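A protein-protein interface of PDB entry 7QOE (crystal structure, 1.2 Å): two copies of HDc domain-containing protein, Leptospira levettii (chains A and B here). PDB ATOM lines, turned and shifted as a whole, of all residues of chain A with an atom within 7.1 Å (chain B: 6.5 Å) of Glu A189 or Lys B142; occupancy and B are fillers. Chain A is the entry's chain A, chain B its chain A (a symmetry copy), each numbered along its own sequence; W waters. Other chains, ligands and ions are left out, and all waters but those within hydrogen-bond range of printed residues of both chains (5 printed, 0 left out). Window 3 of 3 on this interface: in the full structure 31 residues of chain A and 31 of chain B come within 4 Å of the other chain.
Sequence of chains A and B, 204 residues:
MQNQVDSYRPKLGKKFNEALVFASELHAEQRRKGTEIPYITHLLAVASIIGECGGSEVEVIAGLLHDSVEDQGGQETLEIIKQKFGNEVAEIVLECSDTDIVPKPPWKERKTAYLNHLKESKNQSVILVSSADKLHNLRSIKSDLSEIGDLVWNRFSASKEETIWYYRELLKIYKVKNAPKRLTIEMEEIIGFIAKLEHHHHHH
The side-chain amino group (NZ) of Lys A142 lies within salt-bridge range of the side-chain carboxylate (OE1) of Glu B189 (2.8 Å).
NH1 of Arg A182 is in salt-bridge range of OD1 of Asp B144 (3.0 Å).
The side-chain carboxylate (OE1) of Glu B147 is in salt-bridge range of the guanidinium group (NH1) of Arg A182 (2.7 Å).
The side-chain amino group of Lys B142 lies within salt-bridge range of the side-chain carboxylate of Glu A189.
The backbone carbonyl oxygen of Arg B139 is in hydrogen-bond range of the side-chain hydroxyl of Ser B143 (3.2 Å).
The side-chain hydroxyl of Ser B146 sits at hydrogen-bond distance from the backbone carbonyl oxygen of Ser B143 (2.7 Å).
Among the printed residues, merely in contact across the chains: Arg A182 with Ser B143, Arg A182 with Ser B146 and Ile A185 with Ser B146.
Of the printed residues of chain B, Lys A142 touches Glu B189.
Of the printed residues of chain B, Glu A189 touches Lys B142.
Of the printed residues of chain A, Lys B142 touches Glu A189.
Of the printed residues of chain A, Asp B144 touches Arg A182.
Of the printed residues of chain A, Ser B146 touches Arg A182 and Ile A185.
Of the printed residues of chain A, Glu B147 touches Arg A182 (2.7 Å).
The nearest printed residue of chain A that does not touch Asp B144 is Glu A186 (8.3 Å).
Of the 16 printed residues of chain B, 6 touch a printed residue of chain A.
Of the 16 printed residues of chain A, 4 touch a printed residue of chain B.
Printed residues of chain A that touch a printed residue of chain B: Lys A142, Arg A182, Ile A185 and Glu A189.
Hydrophobic or aromatic side chains of chain A that line the printed part of chain B: Ile A185.
Among the printed residues, Asp or Glu carboxylates within 4 Å of a Lys or Arg side-chain nitrogen of the other chain: Lys A142 with Glu B189 (2.8 Å), Arg A182 with Asp B144 (3.0 Å), Arg A182 with Glu B147 (2.7 Å) and Glu A189 with Lys B142 (2.8 Å).
Lys A142 touches Glu B189, and with the chains exchanged Glu A189 touches Lys B142.
Water W4 bridges the side-chain carboxylate of Glu B147 and the backbone NH of Arg A182.
Water W5 lies within hydrogen-bond range of the backbone carbonyl oxygen (O) of Arg A182 (2.7 Å) and the side-chain hydroxyl (OG) of Ser B146 (2.8 Å).
Water W1 lies within hydrogen-bond range of OE1 of Glu A186 (2.7 Å), OG of Ser B143 (2.8 Å) and O of Arg A182 (2.8 Å).
Water W2 lies within hydrogen-bond range of OG of Ser B143, OE1 of Glu A186 and O of Arg B139.
Water W3 lies within hydrogen-bond range of the guanidinium group of Arg A182 (3.1 Å) and the side-chain carboxylate of Asp B144 (3.1 Å).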
ATOM      1  N   LYS A 142      16.002  16.083   5.318  1.00  0.00           N
ATOM      2  CA  LYS A 142      14.614  16.528   5.393  1.00  0.00           C
ATOM      3  C   LYS A 142      14.018  16.249   6.771  1.00  0.00           C
ATOM      4  O   LYS A 142      13.373  17.119   7.373  1.00  0.00           O
ATOM      5  CB  LYS A 142      13.819  15.839   4.279  1.00  0.00           C
ATOM      6  CG  LYS A 142      12.351  16.197   4.210  1.00  0.00           C
ATOM      7  CD  LYS A 142      11.710  15.497   3.000  1.00  0.00           C
ATOM      8  CE  LYS A 142      10.202  15.400   3.099  1.00  0.00           C
ATOM      9  NZ  LYS A 142       9.553  16.721   2.908  1.00  0.00           N
ATOM     10  N   LEU A 171      22.157  14.231  -8.936  1.00  0.00           N
ATOM     11  CA  LEU A 171      20.884  13.858  -9.549  1.00  0.00           C
ATOM     12  C   LEU A 171      20.988  13.810 -11.071  1.00  0.00           C
ATOM     13  O   LEU A 171      20.471  12.884 -11.713  1.00  0.00           O
ATOM     14  CB  LEU A 171      19.799  14.853  -9.122  1.00  0.00           C
ATOM     15  CG  LEU A 171      18.406  14.637  -9.726  1.00  0.00           C
ATOM     16  CD1 LEU A 171      17.843  13.269  -9.392  1.00  0.00           C
ATOM     17  CD2 LEU A 171      17.448  15.733  -9.274  1.00  0.00           C
ATOM     18  N   ARG A 182      12.335   5.437  -9.485  1.00  0.00           N
ATOM     19  CA  ARG A 182      11.741   5.529  -8.157  1.00  0.00           C
ATOM     20  C   ARG A 182      12.648   6.317  -7.217  1.00  0.00           C
ATOM     21  O   ARG A 182      12.154   7.028  -6.334  1.00  0.00           O
ATOM     22  CB  ARG A 182      11.364   4.168  -7.580  1.00  0.00           C
ATOM     23  CG  ARG A 182      12.490   3.235  -7.294  1.00  0.00           C
ATOM     24  CD  ARG A 182      11.995   1.872  -6.738  1.00  0.00           C
ATOM     25  NE  ARG A 182      11.625   1.868  -5.321  1.00  0.00           N
ATOM     26  CZ  ARG A 182      10.416   1.603  -4.830  1.00  0.00           C
ATOM     27  NH1 ARG A 182       9.388   1.315  -5.618  1.00  0.00           N
ATOM     28  NH2 ARG A 182      10.238   1.596  -3.513  1.00  0.00           N
ATOM     29  N   LEU A 183      13.975   6.240  -7.421  1.00  0.00           N
ATOM     30  CA  LEU A 183      14.900   6.988  -6.574  1.00  0.00           C
ATOM     31  C   LEU A 183      15.055   8.428  -7.046  1.00  0.00           C
ATOM     32  O   LEU A 183      15.028   9.360  -6.233  1.00  0.00           O
ATOM     33  CB  LEU A 183      16.263   6.303  -6.526  1.00  0.00           C
ATOM     34  CG  LEU A 183      16.287   4.846  -6.080  1.00  0.00           C
ATOM     35  CD1 LEU A 183      17.731   4.378  -5.853  1.00  0.00           C
ATOM     36  CD2 LEU A 183      15.460   4.590  -4.835  1.00  0.00           C
ATOM     37  N   THR A 184      15.250   8.647  -8.351  1.00  0.00           N
ATOM     38  CA  THR A 184      15.531  10.002  -8.807  1.00  0.00           C
ATOM     39  C   THR A 184      14.308  10.910  -8.704  1.00  0.00           C
ATOM     40  O   THR A 184      14.458  12.115  -8.471  1.00  0.00           O
ATOM     41  CB  THR A 184      16.113  10.006 -10.221  1.00  0.00           C
ATOM     42  OG1 THR A 184      15.217   9.348 -11.128  1.00  0.00           O
ATOM     43  CG2 THR A 184      17.466   9.303 -10.242  1.00  0.00           C
ATOM     44  N   ILE A 185      13.101  10.369  -8.877  1.00  0.00           N
ATOM     45  CA  ILE A 185      11.903  11.182  -8.694  1.00  0.00           C
ATOM     46  C   ILE A 185      11.852  11.728  -7.273  1.00  0.00           C
ATOM     47  O   ILE A 185      11.601  12.920  -7.051  1.00  0.00           O
ATOM     48  CB  ILE A 185      10.637  10.379  -9.036  1.00  0.00           C
ATOM     49  CG1 ILE A 185      10.537  10.191 -10.546  1.00  0.00           C
ATOM     50  CG2 ILE A 185       9.401  11.082  -8.511  1.00  0.00           C
ATOM     51  CD1 ILE A 185       9.622   9.049 -10.963  1.00  0.00           C
ATOM     52  N   GLU A 186      12.073  10.860  -6.287  1.00  0.00           N
ATOM     53  CA  GLU A 186      12.031  11.321  -4.902  1.00  0.00           C
ATOM     54  C   GLU A 186      13.189  12.260  -4.593  1.00  0.00           C
ATOM     55  O   GLU A 186      13.009  13.255  -3.879  1.00  0.00           O
ATOM     56  CB  GLU A 186      11.988  10.137  -3.942  1.00  0.00           C
ATOM     57  CG  GLU A 186      11.692  10.598  -2.522  1.00  0.00           C
ATOM     58  CD  GLU A 186      11.708   9.497  -1.487  1.00  0.00           C
ATOM     59  OE1 GLU A 186      11.808   8.316  -1.852  1.00  0.00           O
ATOM     60  OE2 GLU A 186      11.651   9.819  -0.279  1.00  0.00           O
ATOM     61  N   MET A 187      14.388  11.958  -5.100  1.00  0.00           N
ATOM     62  CA  MET A 187      15.511  12.867  -4.898  1.00  0.00           C
ATOM     63  C   MET A 187      15.138  14.279  -5.320  1.00  0.00           C
ATOM     64  O   MET A 187      15.355  15.248  -4.580  1.00  0.00           O
ATOM     65  CB  MET A 187      16.708  12.428  -5.728  1.00  0.00           C
ATOM     66  CG  MET A 187      17.576  11.386  -5.130  1.00  0.00           C
ATOM     67  SD  MET A 187      19.042  11.237  -6.179  1.00  0.00           S
ATOM     68  CE  MET A 187      19.711   9.724  -5.486  1.00  0.00           C
ATOM     69  N   GLU A 188      14.601  14.414  -6.535  1.00  0.00           N
ATOM     70  CA  GLU A 188      14.291  15.735  -7.063  1.00  0.00           C
ATOM     71  C   GLU A 188      13.291  16.456  -6.168  1.00  0.00           C
ATOM     72  O   GLU A 188      13.414  17.665  -5.943  1.00  0.00           O
ATOM     73  CB  GLU A 188      13.807  15.610  -8.508  1.00  0.00           C
ATOM     74  CG  GLU A 188      13.670  16.934  -9.218  1.00  0.00           C
ATOM     75  CD  GLU A 188      13.762  16.801 -10.727  1.00  0.00           C
ATOM     76  OE1 GLU A 188      13.406  15.728 -11.263  1.00  0.00           O
ATOM     77  OE2 GLU A 188      14.136  17.793 -11.389  1.00  0.00           O
ATOM     78  N   GLU A 189      12.312  15.728  -5.623  1.00  0.00           N
ATOM     79  CA  GLU A 189      11.347  16.352  -4.724  1.00  0.00           C
ATOM     80  C   GLU A 189      12.029  16.856  -3.455  1.00  0.00           C
ATOM     81  O   GLU A 189      11.785  17.984  -3.011  1.00  0.00           O
ATOM     82  CB  GLU A 189      10.238  15.358  -4.371  1.00  0.00           C
ATOM     83  CG  GLU A 189       9.155  15.970  -3.493  1.00  0.00           C
ATOM     84  CD  GLU A 189       7.986  15.036  -3.232  1.00  0.00           C
ATOM     85  OE1 GLU A 189       8.209  13.818  -3.084  1.00  0.00           O
ATOM     86  OE2 GLU A 189       6.839  15.530  -3.176  1.00  0.00           O
ATOM     87  N   ILE A 190      12.887  16.027  -2.855  1.00  0.00           N
ATOM     88  CA  ILE A 190      13.539  16.415  -1.609  1.00  0.00           C
ATOM     89  C   ILE A 190      14.474  17.592  -1.828  1.00  0.00           C
ATOM     90  O   ILE A 190      14.513  18.522  -1.014  1.00  0.00           O
ATOM     91  CB  ILE A 190      14.270  15.227  -0.965  1.00  0.00           C
ATOM     92  CG1 ILE A 190      13.299  14.121  -0.576  1.00  0.00           C
ATOM     93  CG2 ILE A 190      15.013  15.714   0.288  1.00  0.00           C
ATOM     94  CD1 ILE A 190      13.967  12.808  -0.232  1.00  0.00           C
ATOM     95  N   ILE A 191      15.275  17.556  -2.898  1.00  0.00           N
ATOM     96  CA  ILE A 191      16.197  18.655  -3.165  1.00  0.00           C
ATOM     97  C   ILE A 191      15.437  19.973  -3.259  1.00  0.00           C
ATOM     98  O   ILE A 191      15.837  20.988  -2.681  1.00  0.00           O
ATOM     99  CB  ILE A 191      17.032  18.381  -4.427  1.00  0.00           C
ATOM    100  CG1 ILE A 191      18.026  17.241  -4.186  1.00  0.00           C
ATOM    101  CG2 ILE A 191      17.771  19.644  -4.848  1.00  0.00           C
ATOM    102  CD1 ILE A 191      18.585  16.614  -5.460  1.00  0.00           C
ATOM    103  N   GLY A 192      14.329  19.984  -3.999  1.00  0.00           N
ATOM    104  CA  GLY A 192      13.531  21.195  -4.072  1.00  0.00           C
ATOM    105  C   GLY A 192      13.009  21.627  -2.715  1.00  0.00           C
ATOM    106  O   GLY A 192      12.994  22.820  -2.393  1.00  0.00           O
ATOM    107  N   PHE A 193      12.591  20.660  -1.894  1.00  0.00           N
ATOM    108  CA  PHE A 193      12.071  20.967  -0.565  1.00  0.00           C
ATOM    109  C   PHE A 193      13.153  21.575   0.321  1.00  0.00           C
ATOM    110  O   PHE A 193      12.939  22.615   0.951  1.00  0.00           O
ATOM    111  CB  PHE A 193      11.501  19.688   0.058  1.00  0.00           C
ATOM    112  CG  PHE A 193      10.889  19.884   1.410  1.00  0.00           C
ATOM    113  CD1 PHE A 193      11.670  19.841   2.551  1.00  0.00           C
ATOM    114  CD2 PHE A 193       9.528  20.096   1.538  1.00  0.00           C
ATOM    115  CE1 PHE A 193      11.105  20.019   3.797  1.00  0.00           C
ATOM    116  CE2 PHE A 193       8.959  20.278   2.784  1.00  0.00           C
ATOM    117  CZ  PHE A 193       9.751  20.236   3.912  1.00  0.00           C
ATOM    118  N   ILE A 194      14.328  20.943   0.379  1.00  0.00           N
ATOM    119  CA  ILE A 194      15.372  21.420   1.279  1.00  0.00           C
ATOM    120  C   ILE A 194      16.003  22.712   0.777  1.00  0.00           C
ATOM    121  O   ILE A 194      16.550  23.480   1.579  1.00  0.00           O
ATOM    122  CB  ILE A 194      16.395  20.309   1.595  1.00  0.00           C
ATOM    123  CG1 ILE A 194      17.194  19.905   0.363  1.00  0.00           C
ATOM    124  CG2 ILE A 194      15.709  19.097   2.192  1.00  0.00           C
ATOM    125  CD1 ILE A 194      18.477  19.194   0.702  1.00  0.00           C
ATOM    126  N   ALA A 195      15.923  22.992  -0.523  1.00  0.00           N
ATOM    127  CA  ALA A 195      16.385  24.264  -1.059  1.00  0.00           C
ATOM    128  C   ALA A 195      15.464  25.419  -0.688  1.00  0.00           C
ATOM    129  O   ALA A 195      15.761  26.565  -1.050  1.00  0.00           O
ATOM    130  CB  ALA A 195      16.532  24.173  -2.579  1.00  0.00           C
ATOM    131  N   ASN B 137       5.505   1.879   5.327  1.00  0.00           N
ATOM    132  CA  ASN B 137       4.462   1.466   4.397  1.00  0.00           C
ATOM    133  C   ASN B 137       4.004   2.635   3.544  1.00  0.00           C
ATOM    134  O   ASN B 137       3.753   2.470   2.348  1.00  0.00           O
ATOM    135  CB  ASN B 137       3.311   0.829   5.161  1.00  0.00           C
ATOM    136  CG  ASN B 137       3.697  -0.519   5.745  1.00  0.00           C
ATOM    137  OD1 ASN B 137       4.609  -1.180   5.254  1.00  0.00           O
ATOM    138  ND2 ASN B 137       3.000  -0.929   6.787  1.00  0.00           N
ATOM    139  N   LEU B 138       3.880   3.819   4.126  1.00  0.00           N
ATOM    140  CA  LEU B 138       3.460   4.995   3.367  1.00  0.00           C
ATOM    141  C   LEU B 138       4.510   5.419   2.347  1.00  0.00           C
ATOM    142  O   LEU B 138       4.171   5.747   1.200  1.00  0.00           O
ATOM    143  CB  LEU B 138       3.151   6.141   4.329  1.00  0.00           C
ATOM    144  CG  LEU B 138       1.800   6.036   5.038  1.00  0.00           C
ATOM    145  CD1 LEU B 138       1.752   6.978   6.235  1.00  0.00           C
ATOM    146  CD2 LEU B 138       0.648   6.317   4.077  1.00  0.00           C
ATOM    147  N   ARG B 139       5.784   5.435   2.735  1.00  0.00           N
ATOM    148  CA  ARG B 139       6.836   5.745   1.781  1.00  0.00           C
ATOM    149  C   ARG B 139       6.804   4.759   0.625  1.00  0.00           C
ATOM    150  O   ARG B 139       7.040   5.125  -0.532  1.00  0.00           O
ATOM    151  CB  ARG B 139       8.204   5.668   2.460  1.00  0.00           C
ATOM    152  CG  ARG B 139       8.519   6.807   3.420  1.00  0.00           C
ATOM    153  CD  ARG B 139       9.852   6.560   4.077  1.00  0.00           C
ATOM    154  NE  ARG B 139      10.333   7.752   4.767  1.00  0.00           N
ATOM    155  CZ  ARG B 139      11.494   7.822   5.401  1.00  0.00           C
ATOM    156  NH1 ARG B 139      12.285   6.769   5.505  1.00  0.00           N
ATOM    157  NH2 ARG B 139      11.870   8.979   5.944  1.00  0.00           N
ATOM    158  N   SER B 140       6.524   3.496   0.929  1.00  0.00           N
ATOM    159  CA  SER B 140       6.488   2.469  -0.105  1.00  0.00           C
ATOM    160  C   SER B 140       5.338   2.708  -1.078  1.00  0.00           C
ATOM    161  O   SER B 140       5.503   2.529  -2.292  1.00  0.00           O
ATOM    162  CB  SER B 140       6.372   1.109   0.578  1.00  0.00           C
ATOM    163  OG  SER B 140       7.536   0.844   1.363  1.00  0.00           O
ATOM    164  N   ILE B 141       4.159   3.072  -0.584  1.00  0.00           N
ATOM    165  CA  ILE B 141       3.055   3.402  -1.483  1.00  0.00           C
ATOM    166  C   ILE B 141       3.447   4.562  -2.386  1.00  0.00           C
ATOM    167  O   ILE B 141       3.222   4.535  -3.605  1.00  0.00           O
ATOM    168  CB  ILE B 141       1.768   3.720  -0.698  1.00  0.00           C
ATOM    169  CG1 ILE B 141       1.247   2.483   0.031  1.00  0.00           C
ATOM    170  CG2 ILE B 141       0.689   4.288  -1.633  1.00  0.00           C
ATOM    171  CD1 ILE B 141       0.164   2.786   1.049  1.00  0.00           C
ATOM    172  N   LYS B 142       4.002   5.618  -1.799  1.00  0.00           N
ATOM    173  CA  LYS B 142       4.398   6.787  -2.576  1.00  0.00           C
ATOM    174  C   LYS B 142       5.397   6.412  -3.669  1.00  0.00           C
ATOM    175  O   LYS B 142       5.255   6.824  -4.830  1.00  0.00           O
ATOM    176  CB  LYS B 142       4.971   7.839  -1.620  1.00  0.00           C
ATOM    177  CG  LYS B 142       5.428   9.128  -2.268  1.00  0.00           C
ATOM    178  CD  LYS B 142       5.897  10.108  -1.180  1.00  0.00           C
ATOM    179  CE  LYS B 142       6.788  11.209  -1.716  1.00  0.00           C
ATOM    180  NZ  LYS B 142       6.024  12.189  -2.526  1.00  0.00           N
ATOM    181  N   SER B 143       6.434   5.651  -3.318  1.00  0.00           N
ATOM    182  CA  SER B 143       7.406   5.227  -4.321  1.00  0.00           C
ATOM    183  C   SER B 143       6.784   4.366  -5.404  1.00  0.00           C
ATOM    184  O   SER B 143       7.099   4.520  -6.592  1.00  0.00           O
ATOM    185  CB  SER B 143       8.609   4.539  -3.679  1.00  0.00           C
ATOM    186  OG  SER B 143       9.250   5.369  -2.765  1.00  0.00           O
ATOM    187  N   ASP B 144       5.925   3.428  -5.015  1.00  0.00           N
ATOM    188  CA  ASP B 144       5.271   2.587  -6.008  1.00  0.00           C
ATOM    189  C   ASP B 144       4.395   3.425  -6.921  1.00  0.00           C
ATOM    190  O   ASP B 144       4.342   3.173  -8.135  1.00  0.00           O
ATOM    191  CB  ASP B 144       4.480   1.476  -5.326  1.00  0.00           C
ATOM    192  CG  ASP B 144       5.378   0.440  -4.668  1.00  0.00           C
ATOM    193  OD1 ASP B 144       6.558   0.325  -5.071  1.00  0.00           O
ATOM    194  OD2 ASP B 144       4.900  -0.267  -3.748  1.00  0.00           O
ATOM    195  N   LEU B 145       3.684   4.415  -6.380  1.00  0.00           N
ATOM    196  CA  LEU B 145       2.874   5.284  -7.232  1.00  0.00           C
ATOM    197  C   LEU B 145       3.716   5.922  -8.333  1.00  0.00           C
ATOM    198  O   LEU B 145       3.250   6.086  -9.468  1.00  0.00           O
ATOM    199  CB  LEU B 145       2.205   6.374  -6.399  1.00  0.00           C
ATOM    200  CG  LEU B 145       0.945   5.975  -5.641  1.00  0.00           C
ATOM    201  CD1 LEU B 145       0.615   7.019  -4.589  1.00  0.00           C
ATOM    202  CD2 LEU B 145      -0.213   5.785  -6.609  1.00  0.00           C
ATOM    203  N   SER B 146       4.960   6.292  -8.021  1.00  0.00           N
ATOM    204  CA  SER B 146       5.795   6.959  -9.012  1.00  0.00           C
ATOM    205  C   SER B 146       6.220   6.015 -10.128  1.00  0.00           C
ATOM    206  O   SER B 146       6.572   6.486 -11.216  1.00  0.00           O
ATOM    207  CB  SER B 146       7.021   7.598  -8.344  1.00  0.00           C
ATOM    208  OG  SER B 146       8.018   6.642  -8.061  1.00  0.00           O
ATOM    209  N   GLU B 147       6.180   4.704  -9.892  1.00  0.00           N
ATOM    210  CA  GLU B 147       6.562   3.711 -10.885  1.00  0.00           C
ATOM    211  C   GLU B 147       5.374   3.149 -11.657  1.00  0.00           C
ATOM    212  O   GLU B 147       5.427   3.040 -12.889  1.00  0.00           O
ATOM    213  CB  GLU B 147       7.289   2.540 -10.209  1.00  0.00           C
ATOM    214  CG  GLU B 147       8.646   2.869  -9.636  1.00  0.00           C
ATOM    215  CD  GLU B 147       9.425   1.626  -9.224  1.00  0.00           C
ATOM    216  OE1 GLU B 147       9.047   0.970  -8.229  1.00  0.00           O
ATOM    217  OE2 GLU B 147      10.421   1.305  -9.904  1.00  0.00           O
ATOM    218  N   VAL B 152      -0.792   0.435  -8.032  1.00  0.00           N
ATOM    219  CA  VAL B 152      -0.412   0.095  -6.662  1.00  0.00           C
ATOM    220  C   VAL B 152      -1.624  -0.349  -5.852  1.00  0.00           C
ATOM    221  O   VAL B 152      -1.517  -1.217  -4.982  1.00  0.00           O
ATOM    222  CB  VAL B 152       0.329   1.272  -5.991  1.00  0.00           C
ATOM    223  CG1 VAL B 152      -0.617   2.441  -5.729  1.00  0.00           C
ATOM    224  CG2 VAL B 152       0.991   0.834  -4.680  1.00  0.00           C
ATOM    225  N   GLU B 189       2.461  14.492   5.435  1.00  0.00           N
ATOM    226  CA  GLU B 189       2.780  14.921   4.078  1.00  0.00           C
ATOM    227  C   GLU B 189       2.464  13.821   3.068  1.00  0.00           C
ATOM    228  O   GLU B 189       1.858  14.078   2.021  1.00  0.00           O
ATOM    229  CB  GLU B 189       4.254  15.320   3.984  1.00  0.00           C
ATOM    230  CG  GLU B 189       4.636  15.850   2.608  1.00  0.00           C
ATOM    231  CD  GLU B 189       6.063  16.363   2.531  1.00  0.00           C
ATOM    232  OE1 GLU B 189       6.953  15.768   3.172  1.00  0.00           O
ATOM    233  OE2 GLU B 189       6.290  17.368   1.823  1.00  0.00           O
ATOM    234  N   ILE B 190       2.874  12.585   3.366  1.00  0.00           N
ATOM    235  CA  ILE B 190       2.656  11.490   2.429  1.00  0.00           C
ATOM    236  C   ILE B 190       1.174  11.204   2.260  1.00  0.00           C
ATOM    237  O   ILE B 190       0.702  10.978   1.139  1.00  0.00           O
ATOM    238  CB  ILE B 190       3.427  10.230   2.850  1.00  0.00           C
ATOM    239  CG1 ILE B 190       4.932  10.469   2.838  1.00  0.00           C
ATOM    240  CG2 ILE B 190       3.088   9.086   1.883  1.00  0.00           C
ATOM    241  CD1 ILE B 190       5.732   9.390   3.535  1.00  0.00           C
ATOM    242  N   PHE B 193      -0.278  13.566  -0.037  1.00  0.00           N
ATOM    243  CA  PHE B 193       0.204  13.320  -1.393  1.00  0.00           C
ATOM    244  C   PHE B 193      -0.531  12.148  -2.033  1.00  0.00           C
ATOM    245  O   PHE B 193      -1.020  12.254  -3.162  1.00  0.00           O
ATOM    246  CB  PHE B 193       1.715  13.067  -1.349  1.00  0.00           C
ATOM    247  CG  PHE B 193       2.341  12.850  -2.692  1.00  0.00           C
ATOM    248  CD1 PHE B 193       2.358  11.592  -3.267  1.00  0.00           C
ATOM    249  CD2 PHE B 193       2.923  13.904  -3.371  1.00  0.00           C
ATOM    250  CE1 PHE B 193       2.937  11.391  -4.503  1.00  0.00           C
ATOM    251  CE2 PHE B 193       3.501  13.709  -4.612  1.00  0.00           C
ATOM    252  CZ  PHE B 193       3.509  12.449  -5.173  1.00  0.00           C
ATOM    253  N   ILE B 194      -0.624  11.020  -1.326  1.00  0.00           N
ATOM    254  CA  ILE B 194      -1.233   9.834  -1.916  1.00  0.00           C
ATOM    255  C   ILE B 194      -2.745   9.975  -2.039  1.00  0.00           C
ATOM    256  O   ILE B 194      -3.357   9.313  -2.886  1.00  0.00           O
ATOM    257  CB  ILE B 194      -0.785   8.548  -1.190  1.00  0.00           C
ATOM    258  CG1 ILE B 194      -1.303   8.494   0.241  1.00  0.00           C
ATOM    259  CG2 ILE B 194       0.725   8.419  -1.203  1.00  0.00           C
ATOM    260  CD1 ILE B 194      -1.296   7.103   0.817  1.00  0.00           C
HETATM  261  O   HOH W   1      11.674   6.342  -3.660  1.00  0.00           O
HETATM  262  O   HOH W   2       8.470   7.970  -1.853  1.00  0.00           O
HETATM  263  O   HOH W   3       7.948  -0.018  -2.270  1.00  0.00           O
HETATM  264  O   HOH W   4      12.176   2.801 -10.805  1.00  0.00           O
HETATM  265  O   HOH W   5       9.674   7.961  -6.262  1.00  0.00           O
